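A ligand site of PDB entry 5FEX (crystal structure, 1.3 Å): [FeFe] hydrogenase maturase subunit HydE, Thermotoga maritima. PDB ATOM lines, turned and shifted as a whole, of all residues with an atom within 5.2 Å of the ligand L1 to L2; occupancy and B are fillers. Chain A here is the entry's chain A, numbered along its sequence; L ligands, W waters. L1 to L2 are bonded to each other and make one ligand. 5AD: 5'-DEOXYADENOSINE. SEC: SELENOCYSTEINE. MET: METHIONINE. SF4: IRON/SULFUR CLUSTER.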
ATOM      1  N   TYR A  79      25.121   9.750  23.115  1.00  0.00           N
ATOM      2  CA  TYR A  79      24.476   9.786  24.476  1.00  0.00           C
ATOM      3  C   TYR A  79      23.021   9.341  24.481  1.00  0.00           C
ATOM      4  O   TYR A  79      22.439   9.087  25.522  1.00  0.00           O
ATOM      5  CB  TYR A  79      24.566  11.185  25.043  1.00  0.00           C
ATOM      6  CG  TYR A  79      24.237  12.299  24.111  1.00  0.00           C
ATOM      7  CD1 TYR A  79      22.939  12.661  23.846  1.00  0.00           C
ATOM      8  CD2 TYR A  79      25.224  13.032  23.461  1.00  0.00           C
ATOM      9  CE1 TYR A  79      22.657  13.676  22.956  1.00  0.00           C
ATOM     10  CE2 TYR A  79      24.972  14.056  22.571  1.00  0.00           C
ATOM     11  CZ  TYR A  79      23.660  14.376  22.302  1.00  0.00           C
ATOM     12  OH  TYR A  79      23.415  15.378  21.393  1.00  0.00           O
ATOM     13  N   CYS A  80      22.372   9.321  23.290  1.00  0.00           N
ATOM     14  CA  CYS A  80      20.895   9.330  23.254  1.00  0.00           C
ATOM     15  C   CYS A  80      20.263   7.966  22.995  1.00  0.00           C
ATOM     16  O   CYS A  80      20.627   7.258  22.019  1.00  0.00           O
ATOM     17  CB  CYS A  80      20.438  10.217  22.117  1.00  0.00           C
ATOM     18  SG  CYS A  80      18.626  10.432  22.001  1.00  0.00           S
ATOM     19  N   GLY A  81      19.306   7.599  23.826  1.00  0.00           N
ATOM     20  CA  GLY A  81      18.630   6.356  23.646  1.00  0.00           C
ATOM     21  C   GLY A  81      17.836   6.192  22.382  1.00  0.00           C
ATOM     22  O   GLY A  81      17.453   5.067  22.022  1.00  0.00           O
ATOM     23  N   GLN A 117       7.926  17.705  20.244  1.00  0.00           N
ATOM     24  CA  GLN A 117       9.286  17.222  20.228  1.00  0.00           C
ATOM     25  C   GLN A 117       9.346  15.854  19.550  1.00  0.00           C
ATOM     26  O   GLN A 117       8.421  15.041  19.727  1.00  0.00           O
ATOM     27  CB  GLN A 117       9.920  17.153  21.619  1.00  0.00           C
ATOM     28  CG  GLN A 117      11.440  16.871  21.564  1.00  0.00           C
ATOM     29  CD  GLN A 117      12.089  16.862  22.887  1.00  0.00           C
ATOM     30  OE1 GLN A 117      12.066  15.776  23.559  1.00  0.00           O
ATOM     31  NE2 GLN A 117      12.707  17.902  23.307  1.00  0.00           N
ATOM     32  N   ARG A 169      18.980  22.682  21.815  1.00  0.00           N
ATOM     33  CA  ARG A 169      20.112  22.763  22.757  1.00  0.00           C
ATOM     34  C   ARG A 169      21.414  22.753  21.958  1.00  0.00           C
ATOM     35  O   ARG A 169      21.562  21.928  21.029  1.00  0.00           O
ATOM     36  CB  ARG A 169      20.075  21.633  23.750  1.00  0.00           C
ATOM     37  CG  ARG A 169      18.968  21.772  24.754  1.00  0.00           C
ATOM     38  CD  ARG A 169      19.281  20.717  25.816  1.00  0.00           C
ATOM     39  NE  ARG A 169      18.224  20.647  26.751  1.00  0.00           N
ATOM     40  CZ  ARG A 169      18.319  19.932  27.888  1.00  0.00           C
ATOM     41  NH1 ARG A 169      19.363  19.149  28.103  1.00  0.00           N
ATOM     42  NH2 ARG A 169      17.360  20.058  28.769  1.00  0.00           N
ATOM     43  N   GLU A 171      24.165  21.653  23.223  1.00  0.00           N
ATOM     44  CA  GLU A 171      24.676  20.396  23.765  1.00  0.00           C
ATOM     45  C   GLU A 171      26.058  20.547  24.457  1.00  0.00           C
ATOM     46  O   GLU A 171      26.186  20.185  25.614  1.00  0.00           O
ATOM     47  CB  GLU A 171      24.695  19.258  22.700  1.00  0.00           C
ATOM     48  CG  GLU A 171      23.388  19.053  21.924  1.00  0.00           C
ATOM     49  CD  GLU A 171      22.201  18.688  22.750  1.00  0.00           C
ATOM     50  OE1 GLU A 171      22.280  18.638  24.013  1.00  0.00           O
ATOM     51  OE2 GLU A 171      21.105  18.457  22.099  1.00  0.00           O
ATOM     52  N   ARG A 190      25.151  23.320  14.251  1.00  0.00           N
ATOM     53  CA  ARG A 190      24.212  23.577  15.351  1.00  0.00           C
ATOM     54  C   ARG A 190      23.996  25.051  15.588  1.00  0.00           C
ATOM     55  O   ARG A 190      22.887  25.569  15.701  1.00  0.00           O
ATOM     56  CB  ARG A 190      24.707  22.857  16.607  1.00  0.00           C
ATOM     57  CG  ARG A 190      23.647  22.677  17.707  1.00  0.00           C
ATOM     58  CD  ARG A 190      22.691  21.546  17.338  1.00  0.00           C
ATOM     59  NE  ARG A 190      21.879  21.112  18.464  1.00  0.00           N
ATOM     60  CZ  ARG A 190      20.927  20.175  18.377  1.00  0.00           C
ATOM     61  NH1 ARG A 190      20.766  19.485  17.253  1.00  0.00           N
ATOM     62  NH2 ARG A 190      20.195  19.882  19.442  1.00  0.00           N
ATOM     63  N   MET A 209      24.228  19.828  28.141  1.00  0.00           N
ATOM     64  CA  MET A 209      24.314  18.785  29.187  1.00  0.00           C
ATOM     65  C   MET A 209      25.569  19.024  30.047  1.00  0.00           C
ATOM     66  O   MET A 209      26.577  19.612  29.579  1.00  0.00           O
ATOM     67  CB  MET A 209      24.343  17.398  28.601  1.00  0.00           C
ATOM     68  CG  MET A 209      23.000  16.944  28.048  1.00  0.00           C
ATOM     69  SD  MET A 209      23.056  15.355  27.153  1.00  0.00           S
ATOM     70  CE  MET A 209      23.759  15.928  25.643  1.00  0.00           C
ATOM     71  N   PRO A 239      21.657  17.268  33.563  1.00  0.00           N
ATOM     72  CA  PRO A 239      22.785  16.338  33.630  1.00  0.00           C
ATOM     73  C   PRO A 239      22.751  15.319  32.499  1.00  0.00           C
ATOM     74  O   PRO A 239      21.700  14.934  32.049  1.00  0.00           O
ATOM     75  CB  PRO A 239      22.566  15.638  35.003  1.00  0.00           C
ATOM     76  CG  PRO A 239      21.051  15.545  35.078  1.00  0.00           C
ATOM     77  CD  PRO A 239      20.595  16.897  34.505  1.00  0.00           C
ATOM     78  N   PHE A 240      23.973  14.890  32.079  1.00  0.00           N
ATOM     79  CA  PHE A 240      24.076  13.678  31.293  1.00  0.00           C
ATOM     80  C   PHE A 240      23.677  12.470  32.104  1.00  0.00           C
ATOM     81  O   PHE A 240      24.189  12.294  33.225  1.00  0.00           O
ATOM     82  CB  PHE A 240      25.538  13.519  30.797  1.00  0.00           C
ATOM     83  CG  PHE A 240      25.802  12.167  30.222  1.00  0.00           C
ATOM     84  CD1 PHE A 240      25.159  11.668  29.094  1.00  0.00           C
ATOM     85  CD2 PHE A 240      26.780  11.418  30.885  1.00  0.00           C
ATOM     86  CE1 PHE A 240      25.432  10.350  28.643  1.00  0.00           C
ATOM     87  CE2 PHE A 240      27.059  10.108  30.394  1.00  0.00           C
ATOM     88  CZ  PHE A 240      26.390   9.582  29.322  1.00  0.00           C
ATOM     89  N   ILE A 241      22.794  11.625  31.578  1.00  0.00           N
ATOM     90  CA  ILE A 241      22.395  10.401  32.215  1.00  0.00           C
ATOM     91  C   ILE A 241      22.636   9.223  31.247  1.00  0.00           C
ATOM     92  O   ILE A 241      22.039   9.105  30.191  1.00  0.00           O
ATOM     93  CB  ILE A 241      20.898  10.417  32.646  1.00  0.00           C
ATOM     94  CG1 ILE A 241      20.620  11.592  33.637  1.00  0.00           C
ATOM     95  CG2 ILE A 241      20.442   9.074  33.261  1.00  0.00           C
ATOM     96  CD1 ILE A 241      19.127  11.866  33.872  1.00  0.00           C
ATOM     97  N   PRO A 242      23.592   8.325  31.614  1.00  0.00           N
ATOM     98  CA  PRO A 242      23.949   7.259  30.650  1.00  0.00           C
ATOM     99  C   PRO A 242      22.787   6.327  30.369  1.00  0.00           C
ATOM    100  O   PRO A 242      22.029   5.936  31.254  1.00  0.00           O
ATOM    101  CB  PRO A 242      25.106   6.559  31.399  1.00  0.00           C
ATOM    102  CG  PRO A 242      24.810   6.778  32.827  1.00  0.00           C
ATOM    103  CD  PRO A 242      24.255   8.158  32.924  1.00  0.00           C
ATOM    104  N   HIS A 243      22.704   5.908  29.075  1.00  0.00           N
ATOM    105  CA  HIS A 243      21.625   5.036  28.639  1.00  0.00           C
ATOM    106  C   HIS A 243      22.280   3.673  28.253  1.00  0.00           C
ATOM    107  O   HIS A 243      23.283   3.637  27.520  1.00  0.00           O
ATOM    108  CB  HIS A 243      20.923   5.629  27.445  1.00  0.00           C
ATOM    109  CG  HIS A 243      19.682   4.900  27.018  1.00  0.00           C
ATOM    110  ND1 HIS A 243      19.694   3.611  26.517  1.00  0.00           N
ATOM    111  CD2 HIS A 243      18.366   5.276  27.019  1.00  0.00           C
ATOM    112  CE1 HIS A 243      18.464   3.218  26.238  1.00  0.00           C
ATOM    113  NE2 HIS A 243      17.635   4.212  26.539  1.00  0.00           N
ATOM    114  N   THR A 278      14.380  20.967  34.364  1.00  0.00           N
ATOM    115  CA  THR A 278      14.195  19.880  33.388  1.00  0.00           C
ATOM    116  C   THR A 278      13.863  18.558  34.055  1.00  0.00           C
ATOM    117  O   THR A 278      14.192  18.294  35.232  1.00  0.00           O
ATOM    118  CB  THR A 278      15.430  19.755  32.510  1.00  0.00           C
ATOM    119  OG1 THR A 278      16.561  19.420  33.341  1.00  0.00           O
ATOM    120  CG2 THR A 278      15.675  20.994  31.687  1.00  0.00           C
ATOM    121  N   THR A 279      13.170  17.684  33.328  1.00  0.00           N
ATOM    122  CA  THR A 279      12.864  16.419  33.807  1.00  0.00           C
ATOM    123  C   THR A 279      14.144  15.616  34.163  1.00  0.00           C
ATOM    124  O   THR A 279      14.082  14.842  35.152  1.00  0.00           O
ATOM    125  CB  THR A 279      11.990  15.611  32.822  1.00  0.00           C
ATOM    126  OG1 THR A 279      10.733  16.229  32.730  1.00  0.00           O
ATOM    127  CG2 THR A 279      11.758  14.155  33.269  1.00  0.00           C
ATOM    128  N   ALA A 280      15.238  15.785  33.442  1.00  0.00           N
ATOM    129  CA  ALA A 280      16.462  15.076  33.826  1.00  0.00           C
ATOM    130  C   ALA A 280      16.866  15.441  35.236  1.00  0.00           C
ATOM    131  O   ALA A 280      17.397  14.573  36.008  1.00  0.00           O
ATOM    132  CB  ALA A 280      17.559  15.338  32.834  1.00  0.00           C
ATOM    133  N   MET A 281      16.694  16.693  35.659  1.00  0.00           N
ATOM    134  CA  MET A 281      17.022  17.083  37.028  1.00  0.00           C
ATOM    135  C   MET A 281      16.122  16.337  38.032  1.00  0.00           C
ATOM    136  O   MET A 281      16.643  15.956  39.114  1.00  0.00           O
ATOM    137  CB  MET A 281      16.869  18.606  37.212  1.00  0.00           C
ATOM    138  CG  MET A 281      17.970  19.423  36.550  1.00  0.00           C
ATOM    139  SD  MET A 281      19.574  19.145  37.244  1.00  0.00           S
ATOM    140  CE  MET A 281      19.795  20.609  38.294  1.00  0.00           C
ATOM    141  N   MET A 301       7.996  21.664  32.325  1.00  0.00           N
ATOM    142  CA  MET A 301       7.533  21.017  31.120  1.00  0.00           C
ATOM    143  C   MET A 301       6.897  19.628  31.434  1.00  0.00           C
ATOM    144  O   MET A 301       7.540  18.609  31.176  1.00  0.00           O
ATOM    145  CB  MET A 301       8.702  21.020  30.080  1.00  0.00           C
ATOM    146  CG  MET A 301       9.412  22.390  30.072  1.00  0.00           C
ATOM    147  SD  MET A 301      10.809  22.552  28.908  1.00  0.00           S
ATOM    148  CE  MET A 301       9.744  21.636  27.549  1.00  0.00           C
ATOM    149  N   LEU A 315      15.152   9.057  26.246  1.00  0.00           N
ATOM    150  CA  LEU A 315      16.437   9.563  25.864  1.00  0.00           C
ATOM    151  C   LEU A 315      17.446   9.050  26.817  1.00  0.00           C
ATOM    152  O   LEU A 315      18.575   8.799  26.422  1.00  0.00           O
ATOM    153  CB  LEU A 315      16.416  11.111  25.906  1.00  0.00           C
ATOM    154  CG  LEU A 315      15.295  11.873  25.158  1.00  0.00           C
ATOM    155  CD1 LEU A 315      15.568  13.310  25.215  1.00  0.00           C
ATOM    156  CD2 LEU A 315      15.132  11.388  23.835  1.00  0.00           C
ATOM    157  N   TYR A 316      17.005   8.891  28.053  1.00  0.00           N
ATOM    158  CA  TYR A 316      17.763   8.362  29.126  1.00  0.00           C
ATOM    159  C   TYR A 316      16.840   7.523  30.007  1.00  0.00           C
ATOM    160  O   TYR A 316      15.617   7.756  30.005  1.00  0.00           O
ATOM    161  CB  TYR A 316      18.444   9.456  29.985  1.00  0.00           C
ATOM    162  CG  TYR A 316      17.461  10.574  30.401  1.00  0.00           C
ATOM    163  CD1 TYR A 316      16.653  10.418  31.548  1.00  0.00           C
ATOM    164  CD2 TYR A 316      17.328  11.729  29.702  1.00  0.00           C
ATOM    165  CE1 TYR A 316      15.719  11.343  31.959  1.00  0.00           C
ATOM    166  CE2 TYR A 316      16.367  12.691  30.059  1.00  0.00           C
ATOM    167  CZ  TYR A 316      15.554  12.494  31.156  1.00  0.00           C
ATOM    168  OH  TYR A 316      14.614  13.406  31.563  1.00  0.00           O
HETATM  169  N1  5AD L   1      20.998  12.300  29.260  1.00  0.00           N
HETATM  170  C2  5AD L   1      20.424  13.474  29.486  1.00  0.00           C
HETATM  171  N3  5AD L   1      19.951  14.299  28.594  1.00  0.00           N
HETATM  172  C4  5AD L   1      19.840  13.836  27.360  1.00  0.00           C
HETATM  173  N9  5AD L   1      19.418  14.388  26.221  1.00  0.00           N
HETATM  174  C8  5AD L   1      19.571  13.467  25.215  1.00  0.00           C
HETATM  175  N7  5AD L   1      20.112  12.295  25.666  1.00  0.00           N
HETATM  176  C5  5AD L   1      20.318  12.526  27.005  1.00  0.00           C
HETATM  177  C6  5AD L   1      20.872  11.731  28.051  1.00  0.00           C
HETATM  178  N6  5AD L   1      21.383  10.484  27.795  1.00  0.00           N
HETATM  179  C1' 5AD L   1      19.082  15.809  26.140  1.00  0.00           C
HETATM  180  C2' 5AD L   1      19.857  16.526  24.997  1.00  0.00           C
HETATM  181  C3' 5AD L   1      18.719  16.947  24.075  1.00  0.00           C
HETATM  182  C4' 5AD L   1      17.602  17.268  25.145  1.00  0.00           C
HETATM  183  C5' 5AD L   1      16.168  17.308  24.704  1.00  0.00           C
HETATM  184  O4' 5AD L   1      17.716  16.030  25.970  1.00  0.00           O
HETATM  185  O2' 5AD L   1      20.480  17.663  25.638  1.00  0.00           O
HETATM  186  O3' 5AD L   1      18.935  18.199  23.403  1.00  0.00           O
HETATM  187  N   SEC L   2      14.102  18.670  29.155  1.00  0.00           N
HETATM  188  CA  SEC L   2      14.110  17.273  28.671  1.00  0.00           C
HETATM  189  CB  SEC L   2      15.150  16.999  27.628  1.00  0.00           C
HETATM  190 SE   SEC L   2      14.953  18.254  26.095  1.00  0.00          SE
HETATM  191  C   SEC L   2      14.421  16.415  29.816  1.00  0.00           C
HETATM  192  O   SEC L   2      15.168  16.763  30.778  1.00  0.00           O
HETATM  193  OXT SEC L   2      13.904  15.279  29.758  1.00  0.00           O
HETATM  194  N   MET L   3      16.187  15.474  18.275  1.00  0.00           N
HETATM  195  CA  MET L   3      15.986  16.908  18.709  1.00  0.00           C
HETATM  196  C   MET L   3      17.330  17.433  19.129  1.00  0.00           C
HETATM  197  O   MET L   3      17.501  18.659  19.274  1.00  0.00           O
HETATM  198  CB  MET L   3      15.032  16.940  19.882  1.00  0.00           C
HETATM  199  CG  MET L   3      15.619  16.680  21.308  1.00  0.00           C
HETATM  200  SD  MET L   3      16.310  15.045  21.518  1.00  0.00           S
HETATM  201  CE  MET L   3      14.844  14.074  21.447  1.00  0.00           C
HETATM  202  OXT MET L   3      18.283  16.552  19.332  1.00  0.00           O
HETATM  203 FE1  SF4 L   4      18.630  11.761  20.146  1.00  0.00          FE
HETATM  204 FE2  SF4 L   4      18.224  11.950  17.490  1.00  0.00          FE
HETATM  205 FE3  SF4 L   4      20.467  13.040  18.618  1.00  0.00          FE
HETATM  206 FE4  SF4 L   4      17.891  14.343  19.212  1.00  0.00          FE
HETATM  207  S1  SF4 L   4      19.118  14.074  17.092  1.00  0.00           S
HETATM  208  S2  SF4 L   4      19.646  13.755  20.672  1.00  0.00           S
HETATM  209  S3  SF4 L   4      16.689  12.273  19.160  1.00  0.00           S
HETATM  210  S4  SF4 L   4      19.916  10.798  18.464  1.00  0.00           S
HETATM  211  O   HOH W   1      12.006  19.684  27.172  1.00  0.00           O
HETATM  212  O   HOH W   2      17.568  20.008  21.788  1.00  0.00           O
HETATM  213  O   HOH W   3      19.825  16.671  30.176  1.00  0.00           O
HETATM  214  O   HOH W   4      17.573  18.044  30.675  1.00  0.00           O
HETATM  215  O   HOH W   5      13.145  13.691  27.826  1.00  0.00           O
HETATM  216  O   HOH W   6      11.917  18.857  30.978  1.00  0.00           O
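The backbone NH of Met 209 is in hydrogen-bond range of the backbone carbonyl oxygen of Glu 171, 3.2 Å away. OE2 of Glu 171 is in salt-bridge range of NH2 of Arg 190, 3.1 Å away. The backbone NH (N) of Ala 280 lies within hydrogen-bond range of the side-chain hydroxyl (OH) of Tyr 316, 3.1 Å away. The backbone carbonyl oxygen (O) of Arg 169 is in hydrogen-bond range of the guanidinium group (NE) of Arg 190 (2.7 Å). O of Leu 315 lies within hydrogen-bond range of N of Gly 81 (3.0 Å).
An iron atom (FE4) of SF4 L4 is bound by an oxygen (OXT) of MET L3.
Merely in contact with the ligand L1 to L2: Cys 80 (3.9 Å), Gln 117 (3.6 Å), Pro 239 (3.2 Å), Phe 240 (3.9 Å), Thr 278 (3.5 Å) and Leu 315 (3.5 Å). Hydrophobic or aromatic side chains that line the ligand L1 to L2: Tyr 79, Met 209, Ile 241, Ala 280, Leu 315 and Tyr 316. The nearest printed residue that does not touch the ligand L1 to L2 is Arg 190 (4.5 Å).
Water W4 lies within hydrogen-bond range of O of SEC L2 (2.7 Å), NH2 of Arg 169 (2.8 Å) and OG1 of Thr 278 (3.2 Å). Water W2 lies within hydrogen-bond range of an oxygen (O3') of 5AD L1 (2.8 Å), an oxygen (O) of MET L3 (2.9 Å) and the backbone NH (N) of Arg 169 (3.0 Å). Water W6 lies within hydrogen-bond range of N of SEC L2 (2.9 Å) and N of Thr 279 (2.9 Å). Water W3 lies within hydrogen-bond range of a nitrogen (N3) of 5AD L1 (2.9 Å), the backbone carbonyl oxygen of Pro 239 (3.2 Å) and the guanidinium group of Arg 169 (3.3 Å). Water W1 bridges a nitrogen (N) of SEC L2 and the side-chain sulfur (SD) of Met 301.
The side-chain carboxylate (OE2) of Glu 171 sits at hydrogen-bond distance from an oxygen (O3') of 5AD L1 (2.5 Å). An oxygen (OXT) of SEC L2 sits at hydrogen-bond distance from the side-chain hydroxyl (OH) of Tyr 316, at 2.7 Å. The backbone NH (N) of Ala 280 lies within hydrogen-bond range of an oxygen (O) of SEC L2 (2.8 Å). A nitrogen (N1) of 5AD L1 lies within hydrogen-bond range of the backbone NH (N) of Ile 241, at 3.0 Å. The backbone carbonyl oxygen (O) of Ile 241 sits at hydrogen-bond distance from a nitrogen (N6) of 5AD L1 (2.8 Å). A nitrogen (N6) of 5AD L1 lies within hydrogen-bond range of the backbone carbonyl oxygen (O) of Tyr 79 (2.9 Å). O2' of 5AD L1 sits at hydrogen-bond distance from NH1 of Arg 169 (3.1 Å). O of SEC L2 is in hydrogen-bond range of N of Thr 279 (3.4 Å). An oxygen (O2') of 5AD L1 lies close to the side-chain sulfur (SD) of Met 209. An oxygen (O) of MET L3 is in salt-bridge range of the guanidinium group (NH2) of Arg 190, at 3.0 Å. SG of Cys 80 is bound to FE1 of SF4 L4.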
